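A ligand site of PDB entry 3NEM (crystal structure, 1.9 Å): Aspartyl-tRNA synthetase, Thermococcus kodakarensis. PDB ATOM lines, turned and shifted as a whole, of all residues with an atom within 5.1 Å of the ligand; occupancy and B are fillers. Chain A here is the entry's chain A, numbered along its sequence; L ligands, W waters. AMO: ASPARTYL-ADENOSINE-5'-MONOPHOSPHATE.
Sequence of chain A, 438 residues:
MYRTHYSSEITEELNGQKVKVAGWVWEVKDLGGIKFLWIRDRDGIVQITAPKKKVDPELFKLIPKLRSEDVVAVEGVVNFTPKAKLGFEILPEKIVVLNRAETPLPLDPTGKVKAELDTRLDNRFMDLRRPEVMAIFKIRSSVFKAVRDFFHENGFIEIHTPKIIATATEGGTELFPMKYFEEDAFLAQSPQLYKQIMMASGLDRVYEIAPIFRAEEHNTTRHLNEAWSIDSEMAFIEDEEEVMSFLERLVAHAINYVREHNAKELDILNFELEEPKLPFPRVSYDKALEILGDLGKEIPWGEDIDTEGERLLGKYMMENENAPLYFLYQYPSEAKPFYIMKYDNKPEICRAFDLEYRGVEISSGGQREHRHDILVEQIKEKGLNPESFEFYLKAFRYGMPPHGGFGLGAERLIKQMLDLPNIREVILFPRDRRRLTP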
ATOM      1  N   GLU A 170       1.370 -20.873  -4.555  1.00  0.00           N
ATOM      2  CA  GLU A 170       1.023 -19.471  -4.781  1.00  0.00           C
ATOM      3  C   GLU A 170      -0.478 -19.177  -4.670  1.00  0.00           C
ATOM      4  O   GLU A 170      -0.912 -18.052  -4.949  1.00  0.00           O
ATOM      5  CB  GLU A 170       1.512 -18.984  -6.155  1.00  0.00           C
ATOM      6  CG  GLU A 170       3.027 -19.063  -6.350  1.00  0.00           C
ATOM      7  CD  GLU A 170       3.779 -18.125  -5.411  1.00  0.00           C
ATOM      8  OE1 GLU A 170       4.970 -18.368  -5.158  1.00  0.00           O
ATOM      9  OE2 GLU A 170       3.158 -17.137  -4.939  1.00  0.00           O
ATOM     10  N   GLN A 189       3.418 -24.125  -8.595  1.00  0.00           N
ATOM     11  CA  GLN A 189       3.347 -22.834  -9.272  1.00  0.00           C
ATOM     12  C   GLN A 189       4.669 -22.100  -9.100  1.00  0.00           C
ATOM     13  O   GLN A 189       4.960 -21.155  -9.816  1.00  0.00           O
ATOM     14  CB  GLN A 189       2.236 -21.977  -8.651  1.00  0.00           C
ATOM     15  CG  GLN A 189       0.851 -22.552  -8.892  1.00  0.00           C
ATOM     16  CD  GLN A 189      -0.178 -22.035  -7.876  1.00  0.00           C
ATOM     17  OE1 GLN A 189      -1.127 -21.339  -8.228  1.00  0.00           O
ATOM     18  NE2 GLN A 189       0.016 -22.378  -6.618  1.00  0.00           N
ATOM     19  N   SER A 190       5.440 -22.547  -8.115  1.00  0.00           N
ATOM     20  CA  SER A 190       6.696 -21.900  -7.775  1.00  0.00           C
ATOM     21  C   SER A 190       7.366 -22.727  -6.696  1.00  0.00           C
ATOM     22  O   SER A 190       6.727 -23.560  -6.065  1.00  0.00           O
ATOM     23  CB  SER A 190       6.425 -20.526  -7.189  1.00  0.00           C
ATOM     24  OG  SER A 190       5.915 -20.677  -5.879  1.00  0.00           O
ATOM     25  N   GLN A 192       8.386 -21.358  -3.970  1.00  0.00           N
ATOM     26  CA  GLN A 192       8.394 -20.365  -2.900  1.00  0.00           C
ATOM     27  C   GLN A 192       8.529 -20.951  -1.483  1.00  0.00           C
ATOM     28  O   GLN A 192       9.366 -20.528  -0.688  1.00  0.00           O
ATOM     29  CB  GLN A 192       7.135 -19.490  -2.977  1.00  0.00           C
ATOM     30  CG  GLN A 192       7.021 -18.471  -1.833  1.00  0.00           C
ATOM     31  CD  GLN A 192       8.136 -17.445  -1.895  1.00  0.00           C
ATOM     32  OE1 GLN A 192       8.527 -17.015  -2.980  1.00  0.00           O
ATOM     33  NE2 GLN A 192       8.658 -17.057  -0.736  1.00  0.00           N
ATOM     34  N   LYS A 195      12.049 -22.712  -0.977  1.00  0.00           N
ATOM     35  CA  LYS A 195      13.258 -21.888  -0.901  1.00  0.00           C
ATOM     36  C   LYS A 195      13.307 -21.159   0.433  1.00  0.00           C
ATOM     37  O   LYS A 195      14.388 -20.930   0.967  1.00  0.00           O
ATOM     38  CB  LYS A 195      13.418 -20.925  -2.081  1.00  0.00           C
ATOM     39  CG  LYS A 195      12.318 -19.898  -2.257  1.00  0.00           C
ATOM     40  CD  LYS A 195      12.629 -19.018  -3.476  1.00  0.00           C
ATOM     41  CE  LYS A 195      11.565 -17.942  -3.677  1.00  0.00           C
ATOM     42  NZ  LYS A 195      11.969 -17.060  -4.821  1.00  0.00           N
ATOM     43  N   ILE A 212       7.943 -24.177 -13.725  1.00  0.00           N
ATOM     44  CA  ILE A 212       6.796 -23.896 -12.867  1.00  0.00           C
ATOM     45  C   ILE A 212       5.566 -24.126 -13.725  1.00  0.00           C
ATOM     46  O   ILE A 212       5.638 -24.087 -14.951  1.00  0.00           O
ATOM     47  CB  ILE A 212       6.796 -22.435 -12.362  1.00  0.00           C
ATOM     48  CG1 ILE A 212       6.863 -21.441 -13.531  1.00  0.00           C
ATOM     49  CG2 ILE A 212       7.929 -22.214 -11.371  1.00  0.00           C
ATOM     50  CD1 ILE A 212       6.536 -20.000 -13.108  1.00  0.00           C
ATOM     51  N   ARG A 214       1.393 -23.228 -14.221  1.00  0.00           N
ATOM     52  CA  ARG A 214       0.264 -22.384 -13.868  1.00  0.00           C
ATOM     53  C   ARG A 214      -0.837 -22.570 -14.894  1.00  0.00           C
ATOM     54  O   ARG A 214      -0.615 -22.431 -16.107  1.00  0.00           O
ATOM     55  CB  ARG A 214       0.705 -20.931 -13.842  1.00  0.00           C
ATOM     56  CG  ARG A 214       1.988 -20.729 -13.065  1.00  0.00           C
ATOM     57  CD  ARG A 214       1.894 -19.553 -12.156  1.00  0.00           C
ATOM     58  NE  ARG A 214       3.058 -19.419 -11.296  1.00  0.00           N
ATOM     59  CZ  ARG A 214       3.383 -18.271 -10.701  1.00  0.00           C
ATOM     60  NH1 ARG A 214       2.634 -17.196 -10.909  1.00  0.00           N
ATOM     61  NH2 ARG A 214       4.456 -18.194  -9.915  1.00  0.00           N
ATOM     62  N   GLU A 216      -3.239 -21.031 -16.369  1.00  0.00           N
ATOM     63  CA  GLU A 216      -3.780 -19.708 -16.690  1.00  0.00           C
ATOM     64  C   GLU A 216      -5.082 -19.862 -17.463  1.00  0.00           C
ATOM     65  O   GLU A 216      -5.176 -20.651 -18.405  1.00  0.00           O
ATOM     66  CB  GLU A 216      -2.785 -18.898 -17.537  1.00  0.00           C
ATOM     67  CG  GLU A 216      -1.372 -18.685 -16.926  1.00  0.00           C
ATOM     68  CD  GLU A 216      -1.353 -17.697 -15.781  1.00  0.00           C
ATOM     69  OE1 GLU A 216      -2.262 -16.838 -15.716  1.00  0.00           O
ATOM     70  OE2 GLU A 216      -0.417 -17.764 -14.950  1.00  0.00           O
ATOM     71  N   ARG A 222       1.973 -12.914 -23.214  1.00  0.00           N
ATOM     72  CA  ARG A 222       2.997 -12.874 -22.180  1.00  0.00           C
ATOM     73  C   ARG A 222       2.830 -13.908 -21.074  1.00  0.00           C
ATOM     74  O   ARG A 222       3.564 -13.882 -20.088  1.00  0.00           O
ATOM     75  CB  ARG A 222       3.107 -11.454 -21.619  1.00  0.00           C
ATOM     76  CG  ARG A 222       1.766 -10.794 -21.357  1.00  0.00           C
ATOM     77  CD  ARG A 222       1.934  -9.490 -20.594  1.00  0.00           C
ATOM     78  NE  ARG A 222       1.916  -8.301 -21.432  1.00  0.00           N
ATOM     79  CZ  ARG A 222       1.906  -7.056 -20.958  1.00  0.00           C
ATOM     80  NH1 ARG A 222       1.902  -6.857 -19.645  1.00  0.00           N
ATOM     81  NH2 ARG A 222       1.882  -6.026 -21.787  1.00  0.00           N
ATOM     82  N   HIS A 223       1.893 -14.839 -21.226  1.00  0.00           N
ATOM     83  CA  HIS A 223       1.758 -15.929 -20.253  1.00  0.00           C
ATOM     84  C   HIS A 223       1.902 -17.282 -20.923  1.00  0.00           C
ATOM     85  O   HIS A 223       1.559 -17.464 -22.088  1.00  0.00           O
ATOM     86  CB  HIS A 223       0.387 -15.867 -19.558  1.00  0.00           C
ATOM     87  CG  HIS A 223       0.227 -14.698 -18.638  1.00  0.00           C
ATOM     88  ND1 HIS A 223      -0.194 -13.464 -19.080  1.00  0.00           N
ATOM     89  CD2 HIS A 223       0.421 -14.580 -17.307  1.00  0.00           C
ATOM     90  CE1 HIS A 223      -0.252 -12.629 -18.055  1.00  0.00           C
ATOM     91  NE2 HIS A 223       0.112 -13.292 -16.967  1.00  0.00           N
ATOM     92  N   LEU A 224       2.445 -18.243 -20.166  1.00  0.00           N
ATOM     93  CA  LEU A 224       2.440 -19.640 -20.562  1.00  0.00           C
ATOM     94  C   LEU A 224       1.921 -20.444 -19.379  1.00  0.00           C
ATOM     95  O   LEU A 224       1.866 -19.912 -18.267  1.00  0.00           O
ATOM     96  CB  LEU A 224       3.863 -20.101 -20.919  1.00  0.00           C
ATOM     97  CG  LEU A 224       4.543 -19.363 -22.065  1.00  0.00           C
ATOM     98  CD1 LEU A 224       6.065 -19.435 -21.957  1.00  0.00           C
ATOM     99  CD2 LEU A 224       4.053 -19.946 -23.379  1.00  0.00           C
ATOM    100  N   ASN A 225       1.536 -21.693 -19.611  1.00  0.00           N
ATOM    101  CA  ASN A 225       1.093 -22.563 -18.539  1.00  0.00           C
ATOM    102  C   ASN A 225       2.249 -23.393 -17.992  1.00  0.00           C
ATOM    103  O   ASN A 225       2.136 -24.024 -16.944  1.00  0.00           O
ATOM    104  CB  ASN A 225      -0.051 -23.470 -19.002  1.00  0.00           C
ATOM    105  CG  ASN A 225      -1.335 -22.696 -19.269  1.00  0.00           C
ATOM    106  OD1 ASN A 225      -1.413 -21.506 -18.996  1.00  0.00           O
ATOM    107  ND2 ASN A 225      -2.329 -23.375 -19.807  1.00  0.00           N
ATOM    108  N   ALA A 227       6.537 -22.755 -17.564  1.00  0.00           N
ATOM    109  CA  ALA A 227       7.591 -21.760 -17.731  1.00  0.00           C
ATOM    110  C   ALA A 227       8.809 -22.127 -16.912  1.00  0.00           C
ATOM    111  O   ALA A 227       8.746 -23.014 -16.057  1.00  0.00           O
ATOM    112  CB  ALA A 227       7.080 -20.372 -17.329  1.00  0.00           C
ATOM    113  N   SER A 229      11.337 -20.740 -14.159  1.00  0.00           N
ATOM    114  CA  SER A 229      11.527 -19.691 -13.176  1.00  0.00           C
ATOM    115  C   SER A 229      12.941 -19.733 -12.608  1.00  0.00           C
ATOM    116  O   SER A 229      13.439 -20.813 -12.268  1.00  0.00           O
ATOM    117  CB  SER A 229      10.508 -19.855 -12.037  1.00  0.00           C
ATOM    118  OG  SER A 229      10.549 -18.723 -11.183  1.00  0.00           O
ATOM    119  N   ASP A 231      14.705 -18.701  -9.532  1.00  0.00           N
ATOM    120  CA  ASP A 231      14.336 -18.336  -8.172  1.00  0.00           C
ATOM    121  C   ASP A 231      15.566 -18.209  -7.303  1.00  0.00           C
ATOM    122  O   ASP A 231      16.534 -18.939  -7.457  1.00  0.00           O
ATOM    123  CB  ASP A 231      13.414 -19.397  -7.555  1.00  0.00           C
ATOM    124  CG  ASP A 231      11.977 -19.189  -7.921  1.00  0.00           C
ATOM    125  OD1 ASP A 231      11.280 -18.439  -7.172  1.00  0.00           O
ATOM    126  OD2 ASP A 231      11.531 -19.748  -8.956  1.00  0.00           O
ATOM    127  N   SER A 232      15.525 -17.262  -6.374  1.00  0.00           N
ATOM    128  CA  SER A 232      16.602 -17.130  -5.416  1.00  0.00           C
ATOM    129  C   SER A 232      16.005 -16.710  -4.095  1.00  0.00           C
ATOM    130  O   SER A 232      14.950 -16.070  -4.073  1.00  0.00           O
ATOM    131  CB  SER A 232      17.606 -16.078  -5.881  1.00  0.00           C
ATOM    132  OG  SER A 232      18.690 -15.976  -4.968  1.00  0.00           O
ATOM    133  N   GLU A 233      16.676 -17.083  -3.019  1.00  0.00           N
ATOM    134  CA  GLU A 233      16.313 -16.650  -1.676  1.00  0.00           C
ATOM    135  C   GLU A 233      17.633 -16.443  -0.955  1.00  0.00           C
ATOM    136  O   GLU A 233      18.606 -17.184  -1.192  1.00  0.00           O
ATOM    137  CB  GLU A 233      15.451 -17.708  -0.967  1.00  0.00           C
ATOM    138  CG  GLU A 233      14.623 -17.157   0.196  1.00  0.00           C
ATOM    139  CD  GLU A 233      13.465 -16.272  -0.262  1.00  0.00           C
ATOM    140  OE1 GLU A 233      12.925 -15.514   0.576  1.00  0.00           O
ATOM    141  OE2 GLU A 233      13.079 -16.336  -1.450  1.00  0.00           O
ATOM    142  N   TYR A 339       3.318 -14.179   2.446  1.00  0.00           N
ATOM    143  CA  TYR A 339       4.699 -14.456   2.834  1.00  0.00           C
ATOM    144  C   TYR A 339       5.599 -13.227   2.786  1.00  0.00           C
ATOM    145  O   TYR A 339       6.767 -13.296   3.147  1.00  0.00           O
ATOM    146  CB  TYR A 339       5.281 -15.638   2.038  1.00  0.00           C
ATOM    147  CG  TYR A 339       5.151 -15.575   0.530  1.00  0.00           C
ATOM    148  CD1 TYR A 339       5.922 -14.690  -0.220  1.00  0.00           C
ATOM    149  CD2 TYR A 339       4.273 -16.414  -0.151  1.00  0.00           C
ATOM    150  CE1 TYR A 339       5.818 -14.637  -1.601  1.00  0.00           C
ATOM    151  CE2 TYR A 339       4.150 -16.371  -1.539  1.00  0.00           C
ATOM    152  CZ  TYR A 339       4.934 -15.487  -2.254  1.00  0.00           C
ATOM    153  OH  TYR A 339       4.822 -15.448  -3.620  1.00  0.00           O
ATOM    154  N   ILE A 340       5.034 -12.110   2.342  1.00  0.00           N
ATOM    155  CA  ILE A 340       5.763 -10.853   2.295  1.00  0.00           C
ATOM    156  C   ILE A 340       5.659 -10.134   3.647  1.00  0.00           C
ATOM    157  O   ILE A 340       4.602 -10.104   4.284  1.00  0.00           O
ATOM    158  CB  ILE A 340       5.203  -9.938   1.183  1.00  0.00           C
ATOM    159  CG1 ILE A 340       5.281 -10.636  -0.184  1.00  0.00           C
ATOM    160  CG2 ILE A 340       5.970  -8.601   1.161  1.00  0.00           C
ATOM    161  CD1 ILE A 340       6.720 -10.825  -0.730  1.00  0.00           C
ATOM    162  N   GLU A 361       6.222  -7.030 -16.503  1.00  0.00           N
ATOM    163  CA  GLU A 361       6.830  -7.632 -15.318  1.00  0.00           C
ATOM    164  C   GLU A 361       7.707  -8.828 -15.682  1.00  0.00           C
ATOM    165  O   GLU A 361       7.243  -9.777 -16.327  1.00  0.00           O
ATOM    166  CB  GLU A 361       5.752  -8.071 -14.331  1.00  0.00           C
ATOM    167  CG  GLU A 361       6.276  -8.936 -13.189  1.00  0.00           C
ATOM    168  CD  GLU A 361       5.183  -9.658 -12.439  1.00  0.00           C
ATOM    169  OE1 GLU A 361       4.033  -9.162 -12.437  1.00  0.00           O
ATOM    170  OE2 GLU A 361       5.456 -10.713 -11.847  1.00  0.00           O
ATOM    171  N   ILE A 362       8.969  -8.822 -15.255  1.00  0.00           N
ATOM    172  CA  ILE A 362       9.809  -9.998 -15.471  1.00  0.00           C
ATOM    173  C   ILE A 362      10.186 -10.724 -14.172  1.00  0.00           C
ATOM    174  O   ILE A 362      10.621 -11.873 -14.208  1.00  0.00           O
ATOM    175  CB  ILE A 362      11.091  -9.697 -16.276  1.00  0.00           C
ATOM    176  CG1 ILE A 362      11.991  -8.723 -15.517  1.00  0.00           C
ATOM    177  CG2 ILE A 362      10.749  -9.158 -17.681  1.00  0.00           C
ATOM    178  CD1 ILE A 362      13.409  -8.662 -16.097  1.00  0.00           C
ATOM    179  N   SER A 363       9.988 -10.063 -13.039  1.00  0.00           N
ATOM    180  CA  SER A 363      10.275 -10.667 -11.744  1.00  0.00           C
ATOM    181  C   SER A 363       9.445 -10.012 -10.647  1.00  0.00           C
ATOM    182  O   SER A 363       9.066  -8.846 -10.739  1.00  0.00           O
ATOM    183  CB  SER A 363      11.767 -10.520 -11.414  1.00  0.00           C
ATOM    184  OG  SER A 363      12.104 -11.188 -10.209  1.00  0.00           O
ATOM    185  N   SER A 364       9.159 -10.781  -9.610  1.00  0.00           N
ATOM    186  CA  SER A 364       8.618 -10.209  -8.378  1.00  0.00           C
ATOM    187  C   SER A 364       9.350 -10.861  -7.214  1.00  0.00           C
ATOM    188  O   SER A 364       9.900 -11.956  -7.342  1.00  0.00           O
ATOM    189  CB  SER A 364       7.112 -10.446  -8.269  1.00  0.00           C
ATOM    190  OG  SER A 364       6.849 -11.831  -8.153  1.00  0.00           O
ATOM    191  N   GLY A 365       9.363 -10.180  -6.077  1.00  0.00           N
ATOM    192  CA  GLY A 365      10.034 -10.722  -4.905  1.00  0.00           C
ATOM    193  C   GLY A 365       9.775  -9.816  -3.725  1.00  0.00           C
ATOM    194  O   GLY A 365       8.854  -8.995  -3.767  1.00  0.00           O
ATOM    195  N   GLY A 366      10.575  -9.960  -2.675  1.00  0.00           N
ATOM    196  CA  GLY A 366      10.401  -9.141  -1.486  1.00  0.00           C
ATOM    197  C   GLY A 366      11.123  -9.727  -0.296  1.00  0.00           C
ATOM    198  O   GLY A 366      11.678 -10.836  -0.374  1.00  0.00           O
ATOM    199  N   ARG A 368      10.680 -11.523   3.147  1.00  0.00           N
ATOM    200  CA  ARG A 368       9.621 -12.380   3.674  1.00  0.00           C
ATOM    201  C   ARG A 368       9.319 -12.079   5.124  1.00  0.00           C
ATOM    202  O   ARG A 368      10.153 -11.514   5.833  1.00  0.00           O
ATOM    203  CB  ARG A 368      10.008 -13.850   3.568  1.00  0.00           C
ATOM    204  CG  ARG A 368      10.733 -14.223   2.285  1.00  0.00           C
ATOM    205  CD  ARG A 368       9.933 -13.872   1.041  1.00  0.00           C
ATOM    206  NE  ARG A 368      10.674 -14.341  -0.144  1.00  0.00           N
ATOM    207  CZ  ARG A 368      10.335 -14.115  -1.404  1.00  0.00           C
ATOM    208  NH1 ARG A 368       9.232 -13.427  -1.701  1.00  0.00           N
ATOM    209  NH2 ARG A 368      11.106 -14.604  -2.375  1.00  0.00           N
ATOM    210  N   GLY A 405      13.838 -12.719  -1.405  1.00  0.00           N
ATOM    211  CA  GLY A 405      14.219 -13.328  -2.662  1.00  0.00           C
ATOM    212  C   GLY A 405      13.321 -12.881  -3.785  1.00  0.00           C
ATOM    213  O   GLY A 405      12.591 -11.898  -3.660  1.00  0.00           O
ATOM    214  N   PHE A 406      13.382 -13.610  -4.901  1.00  0.00           N
ATOM    215  CA  PHE A 406      12.624 -13.252  -6.081  1.00  0.00           C
ATOM    216  C   PHE A 406      12.421 -14.457  -6.969  1.00  0.00           C
ATOM    217  O   PHE A 406      13.085 -15.475  -6.821  1.00  0.00           O
ATOM    218  CB  PHE A 406      13.347 -12.159  -6.875  1.00  0.00           C
ATOM    219  CG  PHE A 406      14.747 -12.544  -7.298  1.00  0.00           C
ATOM    220  CD1 PHE A 406      15.844 -12.080  -6.596  1.00  0.00           C
ATOM    221  CD2 PHE A 406      14.956 -13.376  -8.391  1.00  0.00           C
ATOM    222  CE1 PHE A 406      17.136 -12.445  -6.985  1.00  0.00           C
ATOM    223  CE2 PHE A 406      16.241 -13.742  -8.785  1.00  0.00           C
ATOM    224  CZ  PHE A 406      17.333 -13.265  -8.079  1.00  0.00           C
ATOM    225  N   GLY A 407      11.467 -14.318  -7.874  1.00  0.00           N
ATOM    226  CA  GLY A 407      11.261 -15.271  -8.955  1.00  0.00           C
ATOM    227  C   GLY A 407      11.389 -14.470 -10.234  1.00  0.00           C
ATOM    228  O   GLY A 407      10.698 -13.462 -10.394  1.00  0.00           O
ATOM    229  N   LEU A 408      12.295 -14.890 -11.107  1.00  0.00           N
ATOM    230  CA  LEU A 408      12.556 -14.194 -12.375  1.00  0.00           C
ATOM    231  C   LEU A 408      12.203 -15.128 -13.526  1.00  0.00           C
ATOM    232  O   LEU A 408      12.785 -16.201 -13.669  1.00  0.00           O
ATOM    233  CB  LEU A 408      14.037 -13.790 -12.427  1.00  0.00           C
ATOM    234  CG  LEU A 408      14.681 -13.339 -13.743  1.00  0.00           C
ATOM    235  CD1 LEU A 408      14.066 -12.036 -14.260  1.00  0.00           C
ATOM    236  CD2 LEU A 408      16.179 -13.174 -13.534  1.00  0.00           C
ATOM    237  N   GLY A 409      11.228 -14.732 -14.337  1.00  0.00           N
ATOM    238  CA  GLY A 409      10.762 -15.621 -15.392  1.00  0.00           C
ATOM    239  C   GLY A 409      11.776 -15.647 -16.519  1.00  0.00           C
ATOM    240  O   GLY A 409      12.132 -14.593 -17.035  1.00  0.00           O
ATOM    241  N   ARG A 412       9.950 -14.589 -19.680  1.00  0.00           N
ATOM    242  CA  ARG A 412       9.655 -13.159 -19.583  1.00  0.00           C
ATOM    243  C   ARG A 412      10.927 -12.333 -19.844  1.00  0.00           C
ATOM    244  O   ARG A 412      10.917 -11.379 -20.612  1.00  0.00           O
ATOM    245  CB  ARG A 412       9.079 -12.809 -18.213  1.00  0.00           C
ATOM    246  CG  ARG A 412       7.626 -13.200 -18.056  1.00  0.00           C
ATOM    247  CD  ARG A 412       6.693 -12.141 -18.644  1.00  0.00           C
ATOM    248  NE  ARG A 412       5.299 -12.545 -18.466  1.00  0.00           N
ATOM    249  CZ  ARG A 412       4.588 -12.332 -17.370  1.00  0.00           C
ATOM    250  NH1 ARG A 412       5.114 -11.670 -16.344  1.00  0.00           N
ATOM    251  NH2 ARG A 412       3.333 -12.764 -17.293  1.00  0.00           N
ATOM    252  N   ILE A 423       5.558 -14.316 -26.220  1.00  0.00           N
ATOM    253  CA  ILE A 423       6.365 -15.143 -25.336  1.00  0.00           C
ATOM    254  C   ILE A 423       6.609 -16.556 -25.894  1.00  0.00           C
ATOM    255  O   ILE A 423       7.547 -17.241 -25.489  1.00  0.00           O
ATOM    256  CB  ILE A 423       5.729 -15.236 -23.931  1.00  0.00           C
ATOM    257  CG1 ILE A 423       6.766 -15.730 -22.925  1.00  0.00           C
ATOM    258  CG2 ILE A 423       4.491 -16.118 -23.973  1.00  0.00           C
ATOM    259  CD1 ILE A 423       6.368 -15.496 -21.467  1.00  0.00           C
HETATM  260  P   AMO L   1       5.201 -14.490  -9.452  1.00  0.00           P
HETATM  261  O1P AMO L   1       3.811 -15.170  -9.488  1.00  0.00           O
HETATM  262  O2P AMO L   1       5.116 -13.029  -9.777  1.00  0.00           O
HETATM  263  O3P AMO L   1       5.877 -14.576  -7.992  1.00  0.00           O
HETATM  264  O5' AMO L   1       6.133 -15.246 -10.455  1.00  0.00           O
HETATM  265  C5' AMO L   1       7.432 -14.763 -10.606  1.00  0.00           C
HETATM  266  C4' AMO L   1       7.802 -14.617 -12.049  1.00  0.00           C
HETATM  267  O4' AMO L   1       7.683 -15.858 -12.823  1.00  0.00           O
HETATM  268  C1' AMO L   1       7.037 -15.495 -14.086  1.00  0.00           C
HETATM  269  N9  AMO L   1       5.808 -16.127 -14.376  1.00  0.00           N
HETATM  270  C4  AMO L   1       5.325 -16.557 -15.684  1.00  0.00           C
HETATM  271  N3  AMO L   1       5.930 -16.597 -16.914  1.00  0.00           N
HETATM  272  C2  AMO L   1       5.204 -17.070 -17.987  1.00  0.00           C
HETATM  273  N1  AMO L   1       3.917 -17.476 -17.827  1.00  0.00           N
HETATM  274  C6  AMO L   1       3.331 -17.443 -16.607  1.00  0.00           C
HETATM  275  N6  AMO L   1       1.983 -17.856 -16.407  1.00  0.00           N
HETATM  276  C5  AMO L   1       4.048 -16.967 -15.502  1.00  0.00           C
HETATM  277  N7  AMO L   1       3.692 -16.808 -14.136  1.00  0.00           N
HETATM  278  C8  AMO L   1       4.828 -16.276 -13.466  1.00  0.00           C
HETATM  279  C2' AMO L   1       7.338 -14.006 -14.253  1.00  0.00           C
HETATM  280  C3' AMO L   1       7.183 -13.510 -12.852  1.00  0.00           C
HETATM  281  O3' AMO L   1       7.521 -12.190 -12.595  1.00  0.00           O
HETATM  282  N   AMO L   1       7.143 -16.868  -5.439  1.00  0.00           N
HETATM  283  CA  AMO L   1       6.983 -15.607  -6.122  1.00  0.00           C
HETATM  284  CB  AMO L   1       8.289 -14.921  -6.421  1.00  0.00           C
HETATM  285  CG  AMO L   1       9.025 -14.401  -5.220  1.00  0.00           C
HETATM  286  OD1 AMO L   1      10.130 -14.846  -4.938  1.00  0.00           O
HETATM  287  OD2 AMO L   1       8.338 -13.632  -4.304  1.00  0.00           O
HETATM  288  C   AMO L   1       6.064 -15.667  -7.335  1.00  0.00           C
HETATM  289  O   AMO L   1       5.829 -16.786  -7.870  1.00  0.00           O
HETATM  290  O2' AMO L   1       8.447 -13.571 -14.955  1.00  0.00           O
HETATM  291  O   HOH W   1       8.716 -18.061  -7.476  1.00  0.00           O
HETATM  292  O   HOH W   2       2.378 -15.106  -6.716  1.00  0.00           O
HETATM  293  O   HOH W   3       6.385 -12.138  -5.360  1.00  0.00           O
HETATM  294  O   HOH W   4       8.792 -16.640 -17.816  1.00  0.00           O
HETATM  295  O   HOH W   5       8.190 -18.086 -10.153  1.00  0.00           O
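Water W3 lies within hydrogen-bond range of OD2 of the ligand (2.7 Å) and OG of Ser 364 (2.8 Å). Water W1 bridges OD1 of Asp 231 (2.6 Å) and N of the ligand (2.8 Å). Water W4 bridges N3 of the ligand (3.0 Å) and N of Arg 412 (3.0 Å). Water W2 bridges OE2 of Glu 170 (2.8 Å) and O1P of the ligand (3.1 Å).
Ser 190 touches the ligand. His 223 touches the ligand. Ala 227 touches the ligand. CA of Gly 365 touches OD2 of the ligand (3.4 Å). Gly 405 touches the ligand. CG of Arg 412 touches O2' of the ligand (3.2 Å). Ile 423 touches the ligand (CD1 to C2, 3.99 Å). Hydrophobic or aromatic side chains within 4 Å of the ligand: His 223, Ala 227, Tyr 339 and Ile 423. 22 residues have an atom within 4 Å of the ligand: Glu 170, Ser 190, Gln 192, Lys 195, Arg 214, Glu 216, His 223, Leu 224, Ala 227, Tyr 339, Glu 361, Ile 362, Ser 363, Ser 364, Gly 365, Arg 368, Gly 405, Phe 406, Gly 407, Gly 409, Arg 412 and Ile 423.
O3' of the ligand sits close to N of Ser 363, 3.3 Å away. A nitrogen (N1) of the ligand lies within hydrogen-bond range of the backbone NH of Leu 224, 2.9 Å away. O2' of the ligand is in hydrogen-bond range of N of Gly 409 (3.1 Å). N6 of the ligand is in hydrogen-bond range of O of Leu 224 (2.8 Å). An oxygen (O2P) of the ligand is in hydrogen-bond range of the side-chain hydroxyl (OG) of Ser 364, 2.7 Å away. An oxygen (OD1) of the ligand is in salt-bridge range of the side-chain amino group (NZ) of Lys 195 (2.9 Å). OD1 of the ligand is in salt-bridge range of NH2 of Arg 368, at 2.8 Å. OE2 of Glu 216 is in hydrogen-bond range of N6 of the ligand (2.8 Å). N of the ligand is in hydrogen-bond range of OE1 of Gln 192, 2.8 Å away. OE2 of Glu 361 lies within hydrogen-bond range of O3' of the ligand (2.6 Å). The backbone NH of Gly 407 lies within hydrogen-bond range of an oxygen (OD1) of the ligand, 3.3 Å away. The side-chain carboxylate (OE1) of Glu 170 lies within salt-bridge range of a nitrogen (N) of the ligand, 2.7 Å away. OH of Tyr 339 lies within hydrogen-bond range of N of the ligand (3.3 Å). N of Phe 406 lies close to OD1 of the ligand, at 3.5 Å. NH1 of Arg 214 lies within salt-bridge range of O1P of the ligand (2.7 Å). The backbone carbonyl oxygen (O) of Ile 362 is in hydrogen-bond range of an oxygen (O2') of the ligand (2.9 Å).
The backbone carbonyl oxygen (O) of Gly 405 lies within hydrogen-bond range of the backbone NH (N) of Gly 366 (3.0 Å). The backbone carbonyl oxygen of Gln 189 lies within hydrogen-bond range of the guanidinium group of Arg 214, at 3.0 Å. The guanidinium group of Arg 368 sits close to the side-chain amide nitrogen of Gln 192, at 3.4 Å. OE2 of Glu 233 is in salt-bridge range of NZ of Lys 195 (3.6 Å). The backbone NH (N) of Gly 407 lies within hydrogen-bond range of the backbone carbonyl oxygen (O) of Ser 364, at 2.9 Å. O of Glu 361 is in hydrogen-bond range of NH1 of Arg 412, 2.8 Å away. The backbone carbonyl oxygen (O) of Gly 407 sits at hydrogen-bond distance from the side-chain hydroxyl (OG) of Ser 363 (2.7 Å). The side-chain amide oxygen of Asn 225 lies within hydrogen-bond range of the backbone NH of Glu 216 (3.2 Å).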
